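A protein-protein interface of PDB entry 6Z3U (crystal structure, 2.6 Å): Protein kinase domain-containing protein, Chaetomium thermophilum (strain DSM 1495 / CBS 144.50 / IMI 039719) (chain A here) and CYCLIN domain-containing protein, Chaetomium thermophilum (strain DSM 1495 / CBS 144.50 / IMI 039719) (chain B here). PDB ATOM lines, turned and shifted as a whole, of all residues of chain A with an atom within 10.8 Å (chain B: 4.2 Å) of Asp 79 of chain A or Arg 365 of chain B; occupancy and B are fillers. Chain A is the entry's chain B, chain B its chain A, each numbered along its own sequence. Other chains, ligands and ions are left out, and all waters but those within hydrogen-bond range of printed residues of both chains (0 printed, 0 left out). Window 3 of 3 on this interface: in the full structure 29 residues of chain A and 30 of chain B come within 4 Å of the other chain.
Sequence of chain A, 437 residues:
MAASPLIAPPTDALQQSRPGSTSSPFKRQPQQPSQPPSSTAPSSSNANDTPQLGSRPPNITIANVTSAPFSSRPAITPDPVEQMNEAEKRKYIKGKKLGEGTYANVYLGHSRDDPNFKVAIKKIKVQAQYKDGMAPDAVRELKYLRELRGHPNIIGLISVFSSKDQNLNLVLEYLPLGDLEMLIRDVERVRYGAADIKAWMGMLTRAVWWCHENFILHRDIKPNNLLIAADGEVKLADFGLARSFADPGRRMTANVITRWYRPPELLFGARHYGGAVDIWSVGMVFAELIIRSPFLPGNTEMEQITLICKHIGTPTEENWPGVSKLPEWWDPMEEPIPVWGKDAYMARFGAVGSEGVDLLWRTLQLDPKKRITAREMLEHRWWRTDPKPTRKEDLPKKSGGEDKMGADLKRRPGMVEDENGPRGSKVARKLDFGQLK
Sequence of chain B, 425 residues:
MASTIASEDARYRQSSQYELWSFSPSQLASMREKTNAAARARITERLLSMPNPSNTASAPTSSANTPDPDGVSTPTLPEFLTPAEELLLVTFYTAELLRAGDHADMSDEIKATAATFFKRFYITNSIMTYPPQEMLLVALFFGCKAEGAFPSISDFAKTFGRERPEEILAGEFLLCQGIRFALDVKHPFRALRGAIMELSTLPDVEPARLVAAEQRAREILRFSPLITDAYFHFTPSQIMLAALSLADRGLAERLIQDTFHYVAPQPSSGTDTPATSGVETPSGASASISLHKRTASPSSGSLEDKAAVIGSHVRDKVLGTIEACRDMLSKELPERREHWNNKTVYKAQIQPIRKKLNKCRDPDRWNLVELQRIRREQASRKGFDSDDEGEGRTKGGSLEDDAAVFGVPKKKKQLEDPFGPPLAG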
ATOM      1  N   PRO A  78       0.255   7.171  17.338  1.00  0.00           N
ATOM      2  CA  PRO A  78       0.853   6.562  16.143  1.00  0.00           C
ATOM      3  C   PRO A  78       2.056   5.674  16.462  1.00  0.00           C
ATOM      4  O   PRO A  78       2.495   4.909  15.602  1.00  0.00           O
ATOM      5  CB  PRO A  78       1.280   7.776  15.304  1.00  0.00           C
ATOM      6  CG  PRO A  78       0.402   8.888  15.765  1.00  0.00           C
ATOM      7  CD  PRO A  78       0.175   8.639  17.230  1.00  0.00           C
ATOM      8  N   ASP A  79       2.573   5.773  17.682  1.00  0.00           N
ATOM      9  CA  ASP A  79       3.756   5.006  18.050  1.00  0.00           C
ATOM     10  C   ASP A  79       3.398   3.526  18.166  1.00  0.00           C
ATOM     11  O   ASP A  79       2.304   3.188  18.628  1.00  0.00           O
ATOM     12  CB  ASP A  79       4.315   5.527  19.376  1.00  0.00           C
ATOM     13  CG  ASP A  79       5.831   5.482  19.438  1.00  0.00           C
ATOM     14  OD1 ASP A  79       6.393   4.374  19.573  1.00  0.00           O
ATOM     15  OD2 ASP A  79       6.458   6.559  19.353  1.00  0.00           O
ATOM     16  N   PRO A  80       4.292   2.616  17.758  1.00  0.00           N
ATOM     17  CA  PRO A  80       3.974   1.184  17.916  1.00  0.00           C
ATOM     18  C   PRO A  80       3.740   0.770  19.359  1.00  0.00           C
ATOM     19  O   PRO A  80       2.845  -0.040  19.629  1.00  0.00           O
ATOM     20  CB  PRO A  80       5.197   0.480  17.305  1.00  0.00           C
ATOM     21  CG  PRO A  80       6.279   1.514  17.279  1.00  0.00           C
ATOM     22  CD  PRO A  80       5.574   2.816  17.061  1.00  0.00           C
ATOM     23  N   VAL A  81       4.526   1.301  20.300  1.00  0.00           N
ATOM     24  CA  VAL A  81       4.293   0.994  21.707  1.00  0.00           C
ATOM     25  C   VAL A  81       3.008   1.648  22.196  1.00  0.00           C
ATOM     26  O   VAL A  81       2.329   1.114  23.080  1.00  0.00           O
ATOM     27  CB  VAL A  81       5.499   1.414  22.569  1.00  0.00           C
ATOM     28  CG1 VAL A  81       6.737   0.634  22.159  1.00  0.00           C
ATOM     29  CG2 VAL A  81       5.749   2.912  22.461  1.00  0.00           C
ATOM     30  N   GLU A  82       2.653   2.811  21.644  1.00  0.00           N
ATOM     31  CA  GLU A  82       1.454   3.497  22.109  1.00  0.00           C
ATOM     32  C   GLU A  82       0.195   2.728  21.727  1.00  0.00           C
ATOM     33  O   GLU A  82      -0.714   2.572  22.550  1.00  0.00           O
ATOM     34  CB  GLU A  82       1.410   4.919  21.552  1.00  0.00           C
ATOM     35  CG  GLU A  82       2.366   5.881  22.243  1.00  0.00           C
ATOM     36  CD  GLU A  82       2.461   7.226  21.545  1.00  0.00           C
ATOM     37  OE1 GLU A  82       1.820   7.398  20.486  1.00  0.00           O
ATOM     38  OE2 GLU A  82       3.180   8.111  22.053  1.00  0.00           O
ATOM     39  N   GLN A  83       0.125   2.226  20.490  1.00  0.00           N
ATOM     40  CA  GLN A  83      -1.031   1.423  20.103  1.00  0.00           C
ATOM     41  C   GLN A  83      -1.048   0.083  20.830  1.00  0.00           C
ATOM     42  O   GLN A  83      -2.127  -0.458  21.100  1.00  0.00           O
ATOM     43  CB  GLN A  83      -1.069   1.220  18.585  1.00  0.00           C
ATOM     44  CG  GLN A  83       0.168   0.598  17.963  1.00  0.00           C
ATOM     45  CD  GLN A  83      -0.016   0.332  16.476  1.00  0.00           C
ATOM     46  OE1 GLN A  83      -1.074  -0.126  16.045  1.00  0.00           O
ATOM     47  NE2 GLN A  83       1.009   0.630  15.685  1.00  0.00           N
ATOM     48  N   MET A  84       0.124  -0.463  21.163  1.00  0.00           N
ATOM     49  CA  MET A  84       0.154  -1.690  21.954  1.00  0.00           C
ATOM     50  C   MET A  84      -0.436  -1.459  23.340  1.00  0.00           C
ATOM     51  O   MET A  84      -1.146  -2.320  23.873  1.00  0.00           O
ATOM     52  CB  MET A  84       1.584  -2.221  22.061  1.00  0.00           C
ATOM     53  CG  MET A  84       1.691  -3.544  22.810  1.00  0.00           C
ATOM     54  SD  MET A  84       3.350  -4.256  22.804  1.00  0.00           S
ATOM     55  CE  MET A  84       3.452  -4.901  21.133  1.00  0.00           C
ATOM     56  N   ASN A  85      -0.152  -0.302  23.943  1.00  0.00           N
ATOM     57  CA  ASN A  85      -0.749   0.015  25.235  1.00  0.00           C
ATOM     58  C   ASN A  85      -2.260   0.162  25.114  1.00  0.00           C
ATOM     59  O   ASN A  85      -3.004  -0.257  26.008  1.00  0.00           O
ATOM     60  CB  ASN A  85      -0.139   1.294  25.809  1.00  0.00           C
ATOM     61  CG  ASN A  85       0.971   1.015  26.811  1.00  0.00           C
ATOM     62  OD1 ASN A  85       0.847   0.135  27.666  1.00  0.00           O
ATOM     63  ND2 ASN A  85       2.057   1.774  26.716  1.00  0.00           N
ATOM     64  N   GLU A  86      -2.733   0.762  24.022  1.00  0.00           N
ATOM     65  CA  GLU A  86      -4.173   0.894  23.838  1.00  0.00           C
ATOM     66  C   GLU A  86      -4.819  -0.470  23.625  1.00  0.00           C
ATOM     67  O   GLU A  86      -5.938  -0.716  24.090  1.00  0.00           O
ATOM     68  CB  GLU A  86      -4.474   1.816  22.657  1.00  0.00           C
ATOM     69  CG  GLU A  86      -3.917   3.230  22.807  1.00  0.00           C
ATOM     70  CD  GLU A  86      -4.106   3.809  24.197  1.00  0.00           C
ATOM     71  OE1 GLU A  86      -5.232   3.734  24.734  1.00  0.00           O
ATOM     72  OE2 GLU A  86      -3.116   4.330  24.757  1.00  0.00           O
ATOM     73  N   ALA A  87      -4.122  -1.373  22.930  1.00  0.00           N
ATOM     74  CA  ALA A  87      -4.627  -2.731  22.768  1.00  0.00           C
ATOM     75  C   ALA A  87      -4.752  -3.442  24.107  1.00  0.00           C
ATOM     76  O   ALA A  87      -5.672  -4.245  24.300  1.00  0.00           O
ATOM     77  CB  ALA A  87      -3.713  -3.522  21.833  1.00  0.00           C
ATOM     78  N   ARG A  90      -7.748  -2.057  26.037  1.00  0.00           N
ATOM     79  CA  ARG A  90      -8.996  -2.596  25.512  1.00  0.00           C
ATOM     80  C   ARG A  90      -9.337  -3.954  26.109  1.00  0.00           C
ATOM     81  O   ARG A  90     -10.498  -4.370  26.046  1.00  0.00           O
ATOM     82  CB  ARG A  90      -8.927  -2.720  23.986  1.00  0.00           C
ATOM     83  CG  ARG A  90      -9.357  -1.466  23.240  1.00  0.00           C
ATOM     84  CD  ARG A  90      -9.558  -1.719  21.742  1.00  0.00           C
ATOM     85  NE  ARG A  90      -8.305  -1.693  20.988  1.00  0.00           N
ATOM     86  CZ  ARG A  90      -7.641  -2.769  20.563  1.00  0.00           C
ATOM     87  NH1 ARG A  90      -8.098  -3.992  20.802  1.00  0.00           N
ATOM     88  NH2 ARG A  90      -6.510  -2.615  19.886  1.00  0.00           N
ATOM     89  N   SER A 162      -0.570   2.057  30.169  1.00  0.00           N
ATOM     90  CA  SER A 162      -0.556   3.504  30.327  1.00  0.00           C
ATOM     91  C   SER A 162      -1.824   4.097  29.727  1.00  0.00           C
ATOM     92  O   SER A 162      -2.315   3.629  28.695  1.00  0.00           O
ATOM     93  CB  SER A 162       0.681   4.108  29.663  1.00  0.00           C
ATOM     94  OG  SER A 162       0.707   3.809  28.281  1.00  0.00           O
ATOM     95  N   LYS A 164      -4.453   7.285  28.314  1.00  0.00           N
ATOM     96  CA  LYS A 164      -4.351   8.360  27.332  1.00  0.00           C
ATOM     97  C   LYS A 164      -3.829   9.645  27.962  1.00  0.00           C
ATOM     98  O   LYS A 164      -3.109  10.409  27.308  1.00  0.00           O
ATOM     99  CB  LYS A 164      -5.711   8.602  26.663  1.00  0.00           C
ATOM    100  CG  LYS A 164      -6.793   9.264  27.534  1.00  0.00           C
ATOM    101  CD  LYS A 164      -7.394   8.311  28.559  1.00  0.00           C
ATOM    102  CE  LYS A 164      -8.521   8.968  29.344  1.00  0.00           C
ATOM    103  NZ  LYS A 164      -9.133   8.033  30.329  1.00  0.00           N
ATOM    104  N   GLN A 166      -1.549   9.943  30.120  1.00  0.00           N
ATOM    105  CA  GLN A 166      -0.211   9.686  30.651  1.00  0.00           C
ATOM    106  C   GLN A 166      -0.256   9.316  32.132  1.00  0.00           C
ATOM    107  O   GLN A 166       0.609   9.708  32.919  1.00  0.00           O
ATOM    108  CB  GLN A 166       0.706  10.888  30.415  1.00  0.00           C
ATOM    109  CG  GLN A 166       0.797  11.297  28.953  1.00  0.00           C
ATOM    110  CD  GLN A 166       1.264  10.164  28.055  1.00  0.00           C
ATOM    111  OE1 GLN A 166       2.338   9.595  28.259  1.00  0.00           O
ATOM    112  NE2 GLN A 166       0.452   9.827  27.057  1.00  0.00           N
ATOM    113  N   ASN B 125      11.837   1.520  20.729  1.00  0.00           N
ATOM    114  CA  ASN B 125      11.778   2.858  20.167  1.00  0.00           C
ATOM    115  C   ASN B 125      13.043   3.109  19.362  1.00  0.00           C
ATOM    116  O   ASN B 125      14.101   2.538  19.644  1.00  0.00           O
ATOM    117  CB  ASN B 125      11.635   3.926  21.257  1.00  0.00           C
ATOM    118  CG  ASN B 125      10.363   3.770  22.057  1.00  0.00           C
ATOM    119  OD1 ASN B 125       9.282   3.595  21.499  1.00  0.00           O
ATOM    120  ND2 ASN B 125      10.487   3.820  23.376  1.00  0.00           N
ATOM    121  N   THR B 129      13.324   8.902  16.986  1.00  0.00           N
ATOM    122  CA  THR B 129      12.073   9.337  17.597  1.00  0.00           C
ATOM    123  C   THR B 129      12.291  10.140  18.876  1.00  0.00           C
ATOM    124  O   THR B 129      11.685  11.201  19.049  1.00  0.00           O
ATOM    125  CB  THR B 129      11.185   8.124  17.895  1.00  0.00           C
ATOM    126  OG1 THR B 129      11.194   7.237  16.769  1.00  0.00           O
ATOM    127  CG2 THR B 129       9.756   8.564  18.168  1.00  0.00           C
ATOM    128  N   TYR B 130      13.138   9.652  19.784  1.00  0.00           N
ATOM    129  CA  TYR B 130      13.400  10.319  21.052  1.00  0.00           C
ATOM    130  C   TYR B 130      14.896  10.538  21.232  1.00  0.00           C
ATOM    131  O   TYR B 130      15.704   9.693  20.825  1.00  0.00           O
ATOM    132  CB  TYR B 130      12.841   9.500  22.223  1.00  0.00           C
ATOM    133  CG  TYR B 130      11.352   9.244  22.132  1.00  0.00           C
ATOM    134  CD1 TYR B 130      10.439  10.280  22.285  1.00  0.00           C
ATOM    135  CD2 TYR B 130      10.860   7.968  21.893  1.00  0.00           C
ATOM    136  CE1 TYR B 130       9.074  10.051  22.206  1.00  0.00           C
ATOM    137  CE2 TYR B 130       9.495   7.728  21.808  1.00  0.00           C
ATOM    138  CZ  TYR B 130       8.607   8.773  21.965  1.00  0.00           C
ATOM    139  OH  TYR B 130       7.251   8.539  21.883  1.00  0.00           O
ATOM    140  N   ASP B 362      12.440  13.179  14.424  1.00  0.00           N
ATOM    141  CA  ASP B 362      11.031  13.523  14.589  1.00  0.00           C
ATOM    142  C   ASP B 362      10.914  14.955  15.097  1.00  0.00           C
ATOM    143  O   ASP B 362      11.508  15.283  16.132  1.00  0.00           O
ATOM    144  CB  ASP B 362      10.369  12.553  15.564  1.00  0.00           C
ATOM    145  CG  ASP B 362       8.856  12.646  15.549  1.00  0.00           C
ATOM    146  OD1 ASP B 362       8.324  13.774  15.514  1.00  0.00           O
ATOM    147  OD2 ASP B 362       8.198  11.583  15.580  1.00  0.00           O
ATOM    148  N   PRO B 363      10.173  15.836  14.417  1.00  0.00           N
ATOM    149  CA  PRO B 363      10.136  17.239  14.861  1.00  0.00           C
ATOM    150  C   PRO B 363       9.301  17.477  16.108  1.00  0.00           C
ATOM    151  O   PRO B 363       9.582  18.428  16.848  1.00  0.00           O
ATOM    152  CB  PRO B 363       9.550  17.974  13.647  1.00  0.00           C
ATOM    153  CG  PRO B 363       8.736  16.948  12.947  1.00  0.00           C
ATOM    154  CD  PRO B 363       9.436  15.635  13.156  1.00  0.00           C
ATOM    155  N   ASP B 364       8.278  16.660  16.365  1.00  0.00           N
ATOM    156  CA  ASP B 364       7.371  16.907  17.482  1.00  0.00           C
ATOM    157  C   ASP B 364       7.824  16.237  18.773  1.00  0.00           C
ATOM    158  O   ASP B 364       7.619  16.790  19.860  1.00  0.00           O
ATOM    159  CB  ASP B 364       5.965  16.427  17.129  1.00  0.00           C
ATOM    160  CG  ASP B 364       5.499  16.948  15.793  1.00  0.00           C
ATOM    161  OD1 ASP B 364       5.503  18.182  15.605  1.00  0.00           O
ATOM    162  OD2 ASP B 364       5.131  16.126  14.931  1.00  0.00           O
ATOM    163  N   ARG B 365       8.420  15.050  18.684  1.00  0.00           N
ATOM    164  CA  ARG B 365       8.775  14.287  19.870  1.00  0.00           C
ATOM    165  C   ARG B 365      10.185  14.554  20.379  1.00  0.00           C
ATOM    166  O   ARG B 365      10.500  14.154  21.506  1.00  0.00           O
ATOM    167  CB  ARG B 365       8.635  12.782  19.605  1.00  0.00           C
ATOM    168  CG  ARG B 365       7.217  12.282  19.382  1.00  0.00           C
ATOM    169  CD  ARG B 365       7.232  10.769  19.177  1.00  0.00           C
ATOM    170  NE  ARG B 365       6.027  10.113  19.681  1.00  0.00           N
ATOM    171  CZ  ARG B 365       4.934   9.855  18.968  1.00  0.00           C
ATOM    172  NH1 ARG B 365       3.907   9.248  19.548  1.00  0.00           N
ATOM    173  NH2 ARG B 365       4.860  10.198  17.688  1.00  0.00           N
ATOM    174  N   TRP B 366      11.042  15.215  19.600  1.00  0.00           N
ATOM    175  CA  TRP B 366      12.422  15.389  20.039  1.00  0.00           C
ATOM    176  C   TRP B 366      12.492  16.248  21.298  1.00  0.00           C
ATOM    177  O   TRP B 366      13.304  15.987  22.193  1.00  0.00           O
ATOM    178  CB  TRP B 366      13.255  16.005  18.919  1.00  0.00           C
ATOM    179  CG  TRP B 366      14.723  15.721  19.038  1.00  0.00           C
ATOM    180  CD1 TRP B 366      15.693  16.567  19.492  1.00  0.00           C
ATOM    181  CD2 TRP B 366      15.388  14.500  18.685  1.00  0.00           C
ATOM    182  NE1 TRP B 366      16.921  15.949  19.442  1.00  0.00           N
ATOM    183  CE2 TRP B 366      16.760  14.681  18.947  1.00  0.00           C
ATOM    184  CE3 TRP B 366      14.955  13.276  18.166  1.00  0.00           C
ATOM    185  CZ2 TRP B 366      17.702  13.679  18.718  1.00  0.00           C
ATOM    186  CZ3 TRP B 366      15.893  12.283  17.936  1.00  0.00           C
ATOM    187  CH2 TRP B 366      17.249  12.491  18.213  1.00  0.00           C
ATOM    188  N   ASN B 367      11.648  17.275  21.386  1.00  0.00           N
ATOM    189  CA  ASN B 367      11.606  18.148  22.558  1.00  0.00           C
ATOM    190  C   ASN B 367      10.683  17.506  23.586  1.00  0.00           C
ATOM    191  O   ASN B 367       9.457  17.595  23.484  1.00  0.00           O
ATOM    192  CB  ASN B 367      11.134  19.547  22.180  1.00  0.00           C
ATOM    193  CG  ASN B 367      11.319  20.545  23.303  1.00  0.00           C
ATOM    194  OD1 ASN B 367      11.274  20.190  24.480  1.00  0.00           O
ATOM    195  ND2 ASN B 367      11.535  21.803  22.946  1.00  0.00           N
ATOM    196  N   LEU B 368      11.282  16.859  24.587  1.00  0.00           N
ATOM    197  CA  LEU B 368      10.493  16.140  25.584  1.00  0.00           C
ATOM    198  C   LEU B 368       9.632  17.091  26.404  1.00  0.00           C
ATOM    199  O   LEU B 368       8.474  16.785  26.709  1.00  0.00           O
ATOM    200  CB  LEU B 368      11.421  15.341  26.496  1.00  0.00           C
ATOM    201  CG  LEU B 368      12.370  14.393  25.764  1.00  0.00           C
ATOM    202  CD1 LEU B 368      13.422  13.866  26.725  1.00  0.00           C
ATOM    203  CD2 LEU B 368      11.605  13.251  25.117  1.00  0.00           C
ATOM    204  N   LEU B 371       6.742  17.914  24.239  1.00  0.00           N
ATOM    205  CA  LEU B 371       5.899  16.728  24.136  1.00  0.00           C
ATOM    206  C   LEU B 371       5.055  16.553  25.392  1.00  0.00           C
ATOM    207  O   LEU B 371       3.859  16.251  25.314  1.00  0.00           O
ATOM    208  CB  LEU B 371       6.767  15.490  23.899  1.00  0.00           C
ATOM    209  CG  LEU B 371       6.145  14.319  23.130  1.00  0.00           C
ATOM    210  CD1 LEU B 371       6.998  13.062  23.293  1.00  0.00           C
ATOM    211  CD2 LEU B 371       4.715  14.051  23.562  1.00  0.00           C
ATOM    212  N   ARG B 375       0.744  17.083  25.791  1.00  0.00           N
ATOM    213  CA  ARG B 375      -0.012  15.917  26.238  1.00  0.00           C
ATOM    214  C   ARG B 375      -0.719  16.172  27.562  1.00  0.00           C
ATOM    215  O   ARG B 375      -1.759  15.558  27.827  1.00  0.00           O
ATOM    216  CB  ARG B 375       0.909  14.699  26.336  1.00  0.00           C
ATOM    217  CG  ARG B 375       1.378  14.207  24.971  1.00  0.00           C
ATOM    218  CD  ARG B 375       1.777  12.739  24.969  1.00  0.00           C
ATOM    219  NE  ARG B 375       1.582  12.150  23.645  1.00  0.00           N
ATOM    220  CZ  ARG B 375       2.205  11.064  23.196  1.00  0.00           C
ATOM    221  NH1 ARG B 375       3.085  10.429  23.959  1.00  0.00           N
ATOM    222  NH2 ARG B 375       1.947  10.615  21.976  1.00  0.00           N
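Hydrophobic or aromatic side chains of chain B that line the printed part of chain A: Tyr 130. Of the 14 printed residues of chain A, 4 touch a printed residue of chain B. Hydrophobic or aromatic side chains of chain A within 4 Å of the printed part of chain B: Val 81. Among the printed residues, 7 pairs touch across the chains. Among the printed residues, Asp or Glu carboxylates within 4 Å of a Lys or Arg side-chain nitrogen of the other chain: Asp 79 of chain A with Arg 365 of chain B (3.6 Å), Glu 82 of chain A with Arg 365 of chain B (2.8 Å) and Glu 82 of chain A with Arg 375 of chain B (2.8 Å).
OH of Tyr 130 of chain B sits at hydrogen-bond distance from OD2 of Asp 79 of chain A (3.3 Å). The side-chain carboxylate (OD2) of Asp 79 of chain A lies within salt-bridge range of the guanidinium group (NE) of Arg 365 of chain B. The guanidinium group (NH1) of Arg 365 of chain B is in salt-bridge range of the side-chain carboxylate (OE2) of Glu 82 of chain A (2.8 Å). OE2 of Glu 82 of chain A lies within salt-bridge range of NH2 of Arg 375 of chain B, 2.8 Å away.
Among the printed residues, merely in contact across the chains: Asp 79 of chain A with Asn 125 of chain B, Val 81 of chain A with Asn 125 of chain B and Gln 166 of chain A with Arg 375 of chain B.
Of the printed residues of chain B, Asp 79 of chain A touches Asn 125 (3.6 Å), Tyr 130 (3.3 Å) and Arg 365 (3.6 Å). Of chain A, only Asp 79 and Glu 82 come within 4 Å of Arg 365 of chain B. No residue of chain A comes within 4 Å of Thr 129 of chain B. No residue of chain A comes within 4 Å of Pro 363 of chain B. Of the printed residues of chain A, Arg 375 of chain B touches Glu 82 and Gln 166. Of the printed residues of chain A, Tyr 130 of chain B touches Asp 79. Met 84 of chain A touches none of the printed residues of chain B. Ser 162 of chain A touches none of the printed residues of chain B. The nearest printed residue of chain B that does not touch Gln 166 of chain A is Leu 371 of chain B (6.9 Å).
The side-chain hydroxyl (OH) of Tyr 130 of chain B lies within hydrogen-bond range of the guanidinium group (NE) of Arg 365 of chain B, at 3.0 Å. The backbone NH of Arg 365 of chain B lies within hydrogen-bond range of the side-chain carboxylate of Asp 362 of chain B, at 3.4 Å. The backbone NH (N) of Asp 79 of chain A lies close to the side-chain carboxylate (OE1) of Glu 82 of chain A (3.3 Å).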
